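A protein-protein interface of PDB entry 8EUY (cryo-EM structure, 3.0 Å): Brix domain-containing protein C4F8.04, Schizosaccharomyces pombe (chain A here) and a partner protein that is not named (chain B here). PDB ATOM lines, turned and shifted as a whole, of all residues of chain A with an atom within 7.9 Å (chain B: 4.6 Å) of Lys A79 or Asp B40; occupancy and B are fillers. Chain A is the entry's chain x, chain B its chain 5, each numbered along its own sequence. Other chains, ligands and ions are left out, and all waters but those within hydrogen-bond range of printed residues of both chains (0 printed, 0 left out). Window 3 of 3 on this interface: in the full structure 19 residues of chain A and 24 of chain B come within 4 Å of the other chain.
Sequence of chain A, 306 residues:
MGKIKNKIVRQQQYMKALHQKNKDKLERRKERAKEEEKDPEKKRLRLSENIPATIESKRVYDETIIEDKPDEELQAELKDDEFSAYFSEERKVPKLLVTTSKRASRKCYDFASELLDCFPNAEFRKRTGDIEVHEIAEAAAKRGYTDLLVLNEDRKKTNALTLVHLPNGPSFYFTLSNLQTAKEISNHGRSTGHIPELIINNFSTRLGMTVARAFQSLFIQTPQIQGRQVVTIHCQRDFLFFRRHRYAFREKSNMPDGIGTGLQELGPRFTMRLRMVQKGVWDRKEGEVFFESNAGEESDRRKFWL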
ATOM      1  N   GLU A  72     -16.370  -7.904  -5.546  1.00  0.00           N
ATOM      2  CA  GLU A  72     -17.790  -8.066  -5.251  1.00  0.00           C
ATOM      3  C   GLU A  72     -18.207  -9.531  -5.222  1.00  0.00           C
ATOM      4  O   GLU A  72     -19.148  -9.884  -4.505  1.00  0.00           O
ATOM      5  CB  GLU A  72     -18.631  -7.287  -6.267  1.00  0.00           C
ATOM      6  CG  GLU A  72     -19.176  -8.110  -7.424  1.00  0.00           C
ATOM      7  CD  GLU A  72     -18.113  -8.476  -8.439  1.00  0.00           C
ATOM      8  OE1 GLU A  72     -16.975  -7.975  -8.324  1.00  0.00           O
ATOM      9  OE2 GLU A  72     -18.417  -9.266  -9.357  1.00  0.00           O
ATOM     10  N   GLU A  73     -17.533 -10.389  -5.991  1.00  0.00           N
ATOM     11  CA  GLU A  73     -17.837 -11.816  -5.938  1.00  0.00           C
ATOM     12  C   GLU A  73     -17.450 -12.408  -4.590  1.00  0.00           C
ATOM     13  O   GLU A  73     -18.195 -13.215  -4.024  1.00  0.00           O
ATOM     14  CB  GLU A  73     -17.122 -12.547  -7.072  1.00  0.00           C
ATOM     15  CG  GLU A  73     -17.550 -13.991  -7.248  1.00  0.00           C
ATOM     16  CD  GLU A  73     -16.915 -14.638  -8.461  1.00  0.00           C
ATOM     17  OE1 GLU A  73     -15.953 -14.060  -9.007  1.00  0.00           O
ATOM     18  OE2 GLU A  73     -17.377 -15.724  -8.870  1.00  0.00           O
ATOM     19  N   LEU A  74     -16.286 -12.020  -4.064  1.00  0.00           N
ATOM     20  CA  LEU A  74     -15.858 -12.520  -2.763  1.00  0.00           C
ATOM     21  C   LEU A  74     -16.792 -12.050  -1.657  1.00  0.00           C
ATOM     22  O   LEU A  74     -17.141 -12.823  -0.758  1.00  0.00           O
ATOM     23  CB  LEU A  74     -14.423 -12.079  -2.482  1.00  0.00           C
ATOM     24  CG  LEU A  74     -13.820 -12.510  -1.145  1.00  0.00           C
ATOM     25  CD1 LEU A  74     -13.523 -13.996  -1.152  1.00  0.00           C
ATOM     26  CD2 LEU A  74     -12.566 -11.713  -0.838  1.00  0.00           C
ATOM     27  N   GLN A  75     -17.208 -10.783  -1.703  1.00  0.00           N
ATOM     28  CA  GLN A  75     -18.120 -10.269  -0.686  1.00  0.00           C
ATOM     29  C   GLN A  75     -19.511 -10.874  -0.816  1.00  0.00           C
ATOM     30  O   GLN A  75     -20.198 -11.062   0.194  1.00  0.00           O
ATOM     31  CB  GLN A  75     -18.193  -8.746  -0.764  1.00  0.00           C
ATOM     32  CG  GLN A  75     -16.885  -8.052  -0.429  1.00  0.00           C
ATOM     33  CD  GLN A  75     -16.326  -8.486   0.912  1.00  0.00           C
ATOM     34  OE1 GLN A  75     -15.238  -9.052   0.991  1.00  0.00           O
ATOM     35  NE2 GLN A  75     -17.073  -8.220   1.976  1.00  0.00           N
ATOM     36  N   ALA A  76     -19.948 -11.172  -2.042  1.00  0.00           N
ATOM     37  CA  ALA A  76     -21.245 -11.813  -2.227  1.00  0.00           C
ATOM     38  C   ALA A  76     -21.257 -13.210  -1.622  1.00  0.00           C
ATOM     39  O   ALA A  76     -22.277 -13.654  -1.085  1.00  0.00           O
ATOM     40  CB  ALA A  76     -21.597 -11.870  -3.712  1.00  0.00           C
ATOM     41  N   GLU A  77     -20.135 -13.923  -1.718  1.00  0.00           N
ATOM     42  CA  GLU A  77     -20.039 -15.243  -1.107  1.00  0.00           C
ATOM     43  C   GLU A  77     -20.115 -15.159   0.411  1.00  0.00           C
ATOM     44  O   GLU A  77     -20.779 -15.981   1.051  1.00  0.00           O
ATOM     45  CB  GLU A  77     -18.739 -15.919  -1.536  1.00  0.00           C
ATOM     46  CG  GLU A  77     -18.882 -16.846  -2.724  1.00  0.00           C
ATOM     47  CD  GLU A  77     -17.807 -17.911  -2.759  1.00  0.00           C
ATOM     48  OE1 GLU A  77     -16.677 -17.629  -2.310  1.00  0.00           O
ATOM     49  OE2 GLU A  77     -18.094 -19.031  -3.230  1.00  0.00           O
ATOM     50  N   LEU A  78     -19.440 -14.173   1.002  1.00  0.00           N
ATOM     51  CA  LEU A  78     -19.321 -14.101   2.454  1.00  0.00           C
ATOM     52  C   LEU A  78     -20.591 -13.591   3.127  1.00  0.00           C
ATOM     53  O   LEU A  78     -20.854 -13.946   4.281  1.00  0.00           O
ATOM     54  CB  LEU A  78     -18.142 -13.204   2.833  1.00  0.00           C
ATOM     55  CG  LEU A  78     -16.764 -13.634   2.334  1.00  0.00           C
ATOM     56  CD1 LEU A  78     -15.708 -12.643   2.785  1.00  0.00           C
ATOM     57  CD2 LEU A  78     -16.427 -15.030   2.815  1.00  0.00           C
ATOM     58  N   LYS A  79     -21.380 -12.763   2.438  1.00  0.00           N
ATOM     59  CA  LYS A  79     -22.501 -12.090   3.087  1.00  0.00           C
ATOM     60  C   LYS A  79     -23.586 -13.054   3.546  1.00  0.00           C
ATOM     61  O   LYS A  79     -24.420 -12.675   4.374  1.00  0.00           O
ATOM     62  CB  LYS A  79     -23.097 -11.037   2.150  1.00  0.00           C
ATOM     63  CG  LYS A  79     -23.758 -11.597   0.906  1.00  0.00           C
ATOM     64  CD  LYS A  79     -25.180 -11.084   0.760  1.00  0.00           C
ATOM     65  CE  LYS A  79     -25.664 -11.215  -0.676  1.00  0.00           C
ATOM     66  NZ  LYS A  79     -27.030 -10.651  -0.862  1.00  0.00           N
ATOM     67  N   ASP A  80     -23.596 -14.281   3.037  1.00  0.00           N
ATOM     68  CA  ASP A  80     -24.524 -15.316   3.478  1.00  0.00           C
ATOM     69  C   ASP A  80     -23.776 -16.612   3.741  1.00  0.00           C
ATOM     70  O   ASP A  80     -24.225 -17.701   3.374  1.00  0.00           O
ATOM     71  CB  ASP A  80     -25.634 -15.530   2.454  1.00  0.00           C
ATOM     72  CG  ASP A  80     -26.598 -14.363   2.388  1.00  0.00           C
ATOM     73  OD1 ASP A  80     -27.026 -13.883   3.458  1.00  0.00           O
ATOM     74  OD2 ASP A  80     -26.927 -13.926   1.265  1.00  0.00           O
ATOM     75  N   ASP A  81     -22.617 -16.509   4.383  1.00  0.00           N
ATOM     76  CA  ASP A  81     -21.731 -17.642   4.594  1.00  0.00           C
ATOM     77  C   ASP A  81     -22.055 -18.312   5.926  1.00  0.00           C
ATOM     78  O   ASP A  81     -23.038 -17.982   6.594  1.00  0.00           O
ATOM     79  CB  ASP A  81     -20.276 -17.182   4.533  1.00  0.00           C
ATOM     80  CG  ASP A  81     -19.434 -18.035   3.611  1.00  0.00           C
ATOM     81  OD1 ASP A  81     -19.899 -18.344   2.496  1.00  0.00           O
ATOM     82  OD2 ASP A  81     -18.303 -18.392   4.001  1.00  0.00           O
ATOM     83  N   GLU A  82     -21.218 -19.270   6.327  1.00  0.00           N
ATOM     84  CA  GLU A  82     -21.404 -19.933   7.611  1.00  0.00           C
ATOM     85  C   GLU A  82     -21.029 -19.023   8.772  1.00  0.00           C
ATOM     86  O   GLU A  82     -21.555 -19.182   9.879  1.00  0.00           O
ATOM     87  CB  GLU A  82     -20.587 -21.222   7.654  1.00  0.00           C
ATOM     88  CG  GLU A  82     -20.649 -22.040   6.370  1.00  0.00           C
ATOM     89  CD  GLU A  82     -19.550 -21.680   5.384  1.00  0.00           C
ATOM     90  OE1 GLU A  82     -18.426 -21.370   5.830  1.00  0.00           O
ATOM     91  OE2 GLU A  82     -19.812 -21.708   4.163  1.00  0.00           O
ATOM     92  N   PHE A  83     -20.131 -18.068   8.544  1.00  0.00           N
ATOM     93  CA  PHE A  83     -19.717 -17.113   9.560  1.00  0.00           C
ATOM     94  C   PHE A  83     -20.437 -15.777   9.430  1.00  0.00           C
ATOM     95  O   PHE A  83     -20.022 -14.797  10.054  1.00  0.00           O
ATOM     96  CB  PHE A  83     -18.205 -16.894   9.494  1.00  0.00           C
ATOM     97  CG  PHE A  83     -17.404 -18.157   9.597  1.00  0.00           C
ATOM     98  CD1 PHE A  83     -17.134 -18.722  10.830  1.00  0.00           C
ATOM     99  CD2 PHE A  83     -16.920 -18.778   8.462  1.00  0.00           C
ATOM    100  CE1 PHE A  83     -16.397 -19.883  10.924  1.00  0.00           C
ATOM    101  CE2 PHE A  83     -16.185 -19.938   8.552  1.00  0.00           C
ATOM    102  CZ  PHE A  83     -15.923 -20.491   9.782  1.00  0.00           C
ATOM    103  N   SER A  84     -21.501 -15.718   8.626  1.00  0.00           N
ATOM    104  CA  SER A  84     -22.169 -14.449   8.358  1.00  0.00           C
ATOM    105  C   SER A  84     -22.820 -13.867   9.606  1.00  0.00           C
ATOM    106  O   SER A  84     -22.913 -12.642   9.736  1.00  0.00           O
ATOM    107  CB  SER A  84     -23.212 -14.630   7.258  1.00  0.00           C
ATOM    108  OG  SER A  84     -24.128 -15.656   7.594  1.00  0.00           O
ATOM    109  N   ALA A  85     -23.273 -14.715  10.528  1.00  0.00           N
ATOM    110  CA  ALA A  85     -23.925 -14.226  11.737  1.00  0.00           C
ATOM    111  C   ALA A  85     -22.980 -13.459  12.651  1.00  0.00           C
ATOM    112  O   ALA A  85     -23.449 -12.785  13.572  1.00  0.00           O
ATOM    113  CB  ALA A  85     -24.548 -15.392  12.503  1.00  0.00           C
ATOM    114  N   PHE A  87     -20.130 -11.472  11.272  1.00  0.00           N
ATOM    115  CA  PHE A  87     -19.638 -10.291  10.579  1.00  0.00           C
ATOM    116  C   PHE A  87     -20.747  -9.372  10.094  1.00  0.00           C
ATOM    117  O   PHE A  87     -20.455  -8.362   9.447  1.00  0.00           O
ATOM    118  CB  PHE A  87     -18.764 -10.706   9.394  1.00  0.00           C
ATOM    119  CG  PHE A  87     -17.508 -11.420   9.792  1.00  0.00           C
ATOM    120  CD1 PHE A  87     -16.374 -10.710  10.136  1.00  0.00           C
ATOM    121  CD2 PHE A  87     -17.466 -12.801   9.827  1.00  0.00           C
ATOM    122  CE1 PHE A  87     -15.221 -11.365  10.501  1.00  0.00           C
ATOM    123  CE2 PHE A  87     -16.316 -13.459  10.192  1.00  0.00           C
ATOM    124  CZ  PHE A  87     -15.192 -12.740  10.530  1.00  0.00           C
ATOM    125  N   SER A  88     -22.004  -9.690  10.379  1.00  0.00           N
ATOM    126  CA  SER A  88     -23.121  -8.859   9.966  1.00  0.00           C
ATOM    127  C   SER A  88     -23.568  -7.977  11.126  1.00  0.00           C
ATOM    128  O   SER A  88     -23.001  -8.003  12.221  1.00  0.00           O
ATOM    129  CB  SER A  88     -24.277  -9.721   9.458  1.00  0.00           C
ATOM    130  OG  SER A  88     -25.093 -10.153  10.531  1.00  0.00           O
ATOM    131  N   ARG A 213     -11.166 -16.093   8.817  1.00  0.00           N
ATOM    132  CA  ARG A 213     -12.517 -15.836   9.307  1.00  0.00           C
ATOM    133  C   ARG A 213     -12.862 -16.754  10.469  1.00  0.00           C
ATOM    134  O   ARG A 213     -13.498 -16.327  11.439  1.00  0.00           O
ATOM    135  CB  ARG A 213     -13.530 -16.015   8.180  1.00  0.00           C
ATOM    136  CG  ARG A 213     -13.587 -14.868   7.197  1.00  0.00           C
ATOM    137  CD  ARG A 213     -14.792 -15.006   6.291  1.00  0.00           C
ATOM    138  NE  ARG A 213     -15.833 -14.038   6.607  1.00  0.00           N
ATOM    139  CZ  ARG A 213     -17.131 -14.276   6.493  1.00  0.00           C
ATOM    140  NH1 ARG A 213     -17.585 -15.454   6.101  1.00  0.00           N
ATOM    141  NH2 ARG A 213     -17.997 -13.307   6.777  1.00  0.00           N
ATOM    142  N   ILE B   9     -23.772 -19.514  -5.212  1.00  0.00           N
ATOM    143  CA  ILE B   9     -24.468 -18.239  -5.092  1.00  0.00           C
ATOM    144  C   ILE B   9     -25.334 -17.950  -6.313  1.00  0.00           C
ATOM    145  O   ILE B   9     -25.762 -16.810  -6.511  1.00  0.00           O
ATOM    146  CB  ILE B   9     -23.485 -17.087  -4.831  1.00  0.00           C
ATOM    147  CG1 ILE B   9     -22.512 -16.929  -5.997  1.00  0.00           C
ATOM    148  CG2 ILE B   9     -22.728 -17.322  -3.539  1.00  0.00           C
ATOM    149  CD1 ILE B   9     -21.495 -15.843  -5.778  1.00  0.00           C
ATOM    150  N   GLY B  10     -25.593 -18.956  -7.142  1.00  0.00           N
ATOM    151  CA  GLY B  10     -26.559 -18.849  -8.209  1.00  0.00           C
ATOM    152  C   GLY B  10     -26.053 -18.262  -9.507  1.00  0.00           C
ATOM    153  O   GLY B  10     -26.814 -18.222 -10.481  1.00  0.00           O
ATOM    154  N   GLU B  38     -27.985 -14.868 -11.101  1.00  0.00           N
ATOM    155  CA  GLU B  38     -28.226 -14.228  -9.818  1.00  0.00           C
ATOM    156  C   GLU B  38     -26.979 -14.290  -8.944  1.00  0.00           C
ATOM    157  O   GLU B  38     -26.168 -15.212  -9.049  1.00  0.00           O
ATOM    158  CB  GLU B  38     -29.401 -14.888  -9.092  1.00  0.00           C
ATOM    159  CG  GLU B  38     -30.087 -13.984  -8.086  1.00  0.00           C
ATOM    160  CD  GLU B  38     -30.273 -12.573  -8.606  1.00  0.00           C
ATOM    161  OE1 GLU B  38     -31.042 -12.391  -9.573  1.00  0.00           O
ATOM    162  OE2 GLU B  38     -29.647 -11.646  -8.051  1.00  0.00           O
ATOM    163  N   LEU B  39     -26.834 -13.291  -8.077  1.00  0.00           N
ATOM    164  CA  LEU B  39     -25.717 -13.201  -7.144  1.00  0.00           C
ATOM    165  C   LEU B  39     -26.194 -13.320  -5.700  1.00  0.00           C
ATOM    166  O   LEU B  39     -25.708 -12.623  -4.808  1.00  0.00           O
ATOM    167  CB  LEU B  39     -24.949 -11.896  -7.344  1.00  0.00           C
ATOM    168  CG  LEU B  39     -23.621 -11.975  -8.099  1.00  0.00           C
ATOM    169  CD1 LEU B  39     -22.534 -12.571  -7.221  1.00  0.00           C
ATOM    170  CD2 LEU B  39     -23.773 -12.771  -9.385  1.00  0.00           C
ATOM    171  N   ASP B  40     -27.153 -14.208  -5.456  1.00  0.00           N
ATOM    172  CA  ASP B  40     -27.726 -14.408  -4.134  1.00  0.00           C
ATOM    173  C   ASP B  40     -27.579 -15.864  -3.719  1.00  0.00           C
ATOM    174  O   ASP B  40     -27.739 -16.773  -4.539  1.00  0.00           O
ATOM    175  CB  ASP B  40     -29.202 -14.003  -4.104  1.00  0.00           C
ATOM    176  CG  ASP B  40     -29.756 -13.927  -2.696  1.00  0.00           C
ATOM    177  OD1 ASP B  40     -29.411 -12.970  -1.972  1.00  0.00           O
ATOM    178  OD2 ASP B  40     -30.533 -14.824  -2.313  1.00  0.00           O
ATOM    179  N   ARG B  41     -27.273 -16.077  -2.438  1.00  0.00           N
ATOM    180  CA  ARG B  41     -27.082 -17.433  -1.933  1.00  0.00           C
ATOM    181  C   ARG B  41     -28.371 -18.243  -1.996  1.00  0.00           C
ATOM    182  O   ARG B  41     -28.346 -19.430  -2.338  1.00  0.00           O
ATOM    183  CB  ARG B  41     -26.549 -17.388  -0.503  1.00  0.00           C
ATOM    184  CG  ARG B  41     -26.317 -18.751   0.117  1.00  0.00           C
ATOM    185  CD  ARG B  41     -25.114 -19.430  -0.505  1.00  0.00           C
ATOM    186  NE  ARG B  41     -23.872 -18.740  -0.178  1.00  0.00           N
ATOM    187  CZ  ARG B  41     -23.015 -19.144   0.747  1.00  0.00           C
ATOM    188  NH1 ARG B  41     -23.230 -20.239   1.456  1.00  0.00           N
ATOM    189  NH2 ARG B  41     -21.914 -18.433   0.965  1.00  0.00           N
ATOM    190  N   GLU B  42     -29.506 -17.621  -1.667  1.00  0.00           N
ATOM    191  CA  GLU B  42     -30.770 -18.349  -1.614  1.00  0.00           C
ATOM    192  C   GLU B  42     -31.216 -18.854  -2.979  1.00  0.00           C
ATOM    193  O   GLU B  42     -32.082 -19.731  -3.046  1.00  0.00           O
ATOM    194  CB  GLU B  42     -31.861 -17.467  -1.004  1.00  0.00           C
ATOM    195  CG  GLU B  42     -31.815 -17.358   0.520  1.00  0.00           C
ATOM    196  CD  GLU B  42     -30.671 -16.497   1.038  1.00  0.00           C
ATOM    197  OE1 GLU B  42     -29.790 -16.109   0.243  1.00  0.00           O
ATOM    198  OE2 GLU B  42     -30.656 -16.209   2.253  1.00  0.00           O
ATOM    199  N   LYS B  43     -30.651 -18.324  -4.062  1.00  0.00           N
ATOM    200  CA  LYS B  43     -30.953 -18.785  -5.410  1.00  0.00           C
ATOM    201  C   LYS B  43     -29.800 -19.590  -6.002  1.00  0.00           C
ATOM    202  O   LYS B  43     -29.568 -19.556  -7.212  1.00  0.00           O
ATOM    203  CB  LYS B  43     -31.299 -17.604  -6.314  1.00  0.00           C
ATOM    204  CG  LYS B  43     -32.689 -17.039  -6.082  1.00  0.00           C
ATOM    205  CD  LYS B  43     -32.980 -15.875  -7.014  1.00  0.00           C
ATOM    206  CE  LYS B  43     -32.968 -16.318  -8.468  1.00  0.00           C
ATOM    207  NZ  LYS B  43     -34.058 -17.287  -8.762  1.00  0.00           N
ATOM    208  N   GLY B  44     -29.070 -20.314  -5.158  1.00  0.00           N
ATOM    209  CA  GLY B  44     -27.946 -21.091  -5.639  1.00  0.00           C
ATOM    210  C   GLY B  44     -28.381 -22.245  -6.519  1.00  0.00           C
ATOM    211  O   GLY B  44     -29.456 -22.819  -6.355  1.00  0.00           O
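The guanidinium group (NH2) of Arg B41 sits at hydrogen-bond distance from the backbone carbonyl oxygen (O) of Glu A77 (2.7 Å). NZ of Lys A79 is in salt-bridge range of OD1 of Asp B40, 3.5 Å away. The guanidinium group of Arg B41 sits close to the backbone carbonyl oxygen of Asp A80, at 3.3 Å. OD1 of Asp A81 lies within salt-bridge range of NH2 of Arg B41, at 2.5 Å.
The side-chain amino group of Lys A79 lies within salt-bridge range of the side-chain carboxylate of Asp A80 (3.9 Å). O of Asp A81 is in hydrogen-bond range of OG of Ser A84 (2.8 Å). The side-chain carboxylate (OD2) of Asp A81 is in salt-bridge range of the guanidinium group (NH1) of Arg A213, 3.7 Å away. The backbone carbonyl oxygen (O) of Ile B9 lies within hydrogen-bond range of the backbone NH (N) of Asp B40 (3.1 Å). The side-chain carboxylate (OD2) of Asp B40 sits at hydrogen-bond distance from the backbone NH (N) of Glu B42, at 3.0 Å.
Leu B39 touches Ala A76 (CD1 to CB, 3.7 Å). Glu A77 touches Ile B9 (CG to CG2, 3.96 Å). Asp A80 touches Glu B42.
Printed residues of chain B within 4 Å of Lys A79: Asp B40 (3.5 Å). Asp B40 touches just one residue of chain A: Lys A79 (3.5 Å). Of the printed residues of chain B, Ala A76 touches Leu B39 (3.7 Å). Printed residues of chain B within 4 Å of Glu A77: Ile B9 (3.96 Å) and Arg B41 (2.7 Å). Phe A87 touches none of the printed residues of chain B. The nearest residue of chain B that does not touch Lys A79 is Leu B39 (4.4 Å). The nearest residue of chain A that does not touch Asp B40 is Asp A80 (4.2 Å). The nearest printed residue of chain A that does not touch Arg B41 is Glu A82 (4.6 Å).
Hydrophobic or aromatic side chains of chain B within 4 Å of the printed part of chain A: Ile B9 and Leu B39. Of the 17 printed residues of chain A, 5 touch a printed residue of chain B. Printed residues of chain A that touch a printed residue of chain B: Ala A76, Glu A77, Lys A79, Asp A80 and Asp A81.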
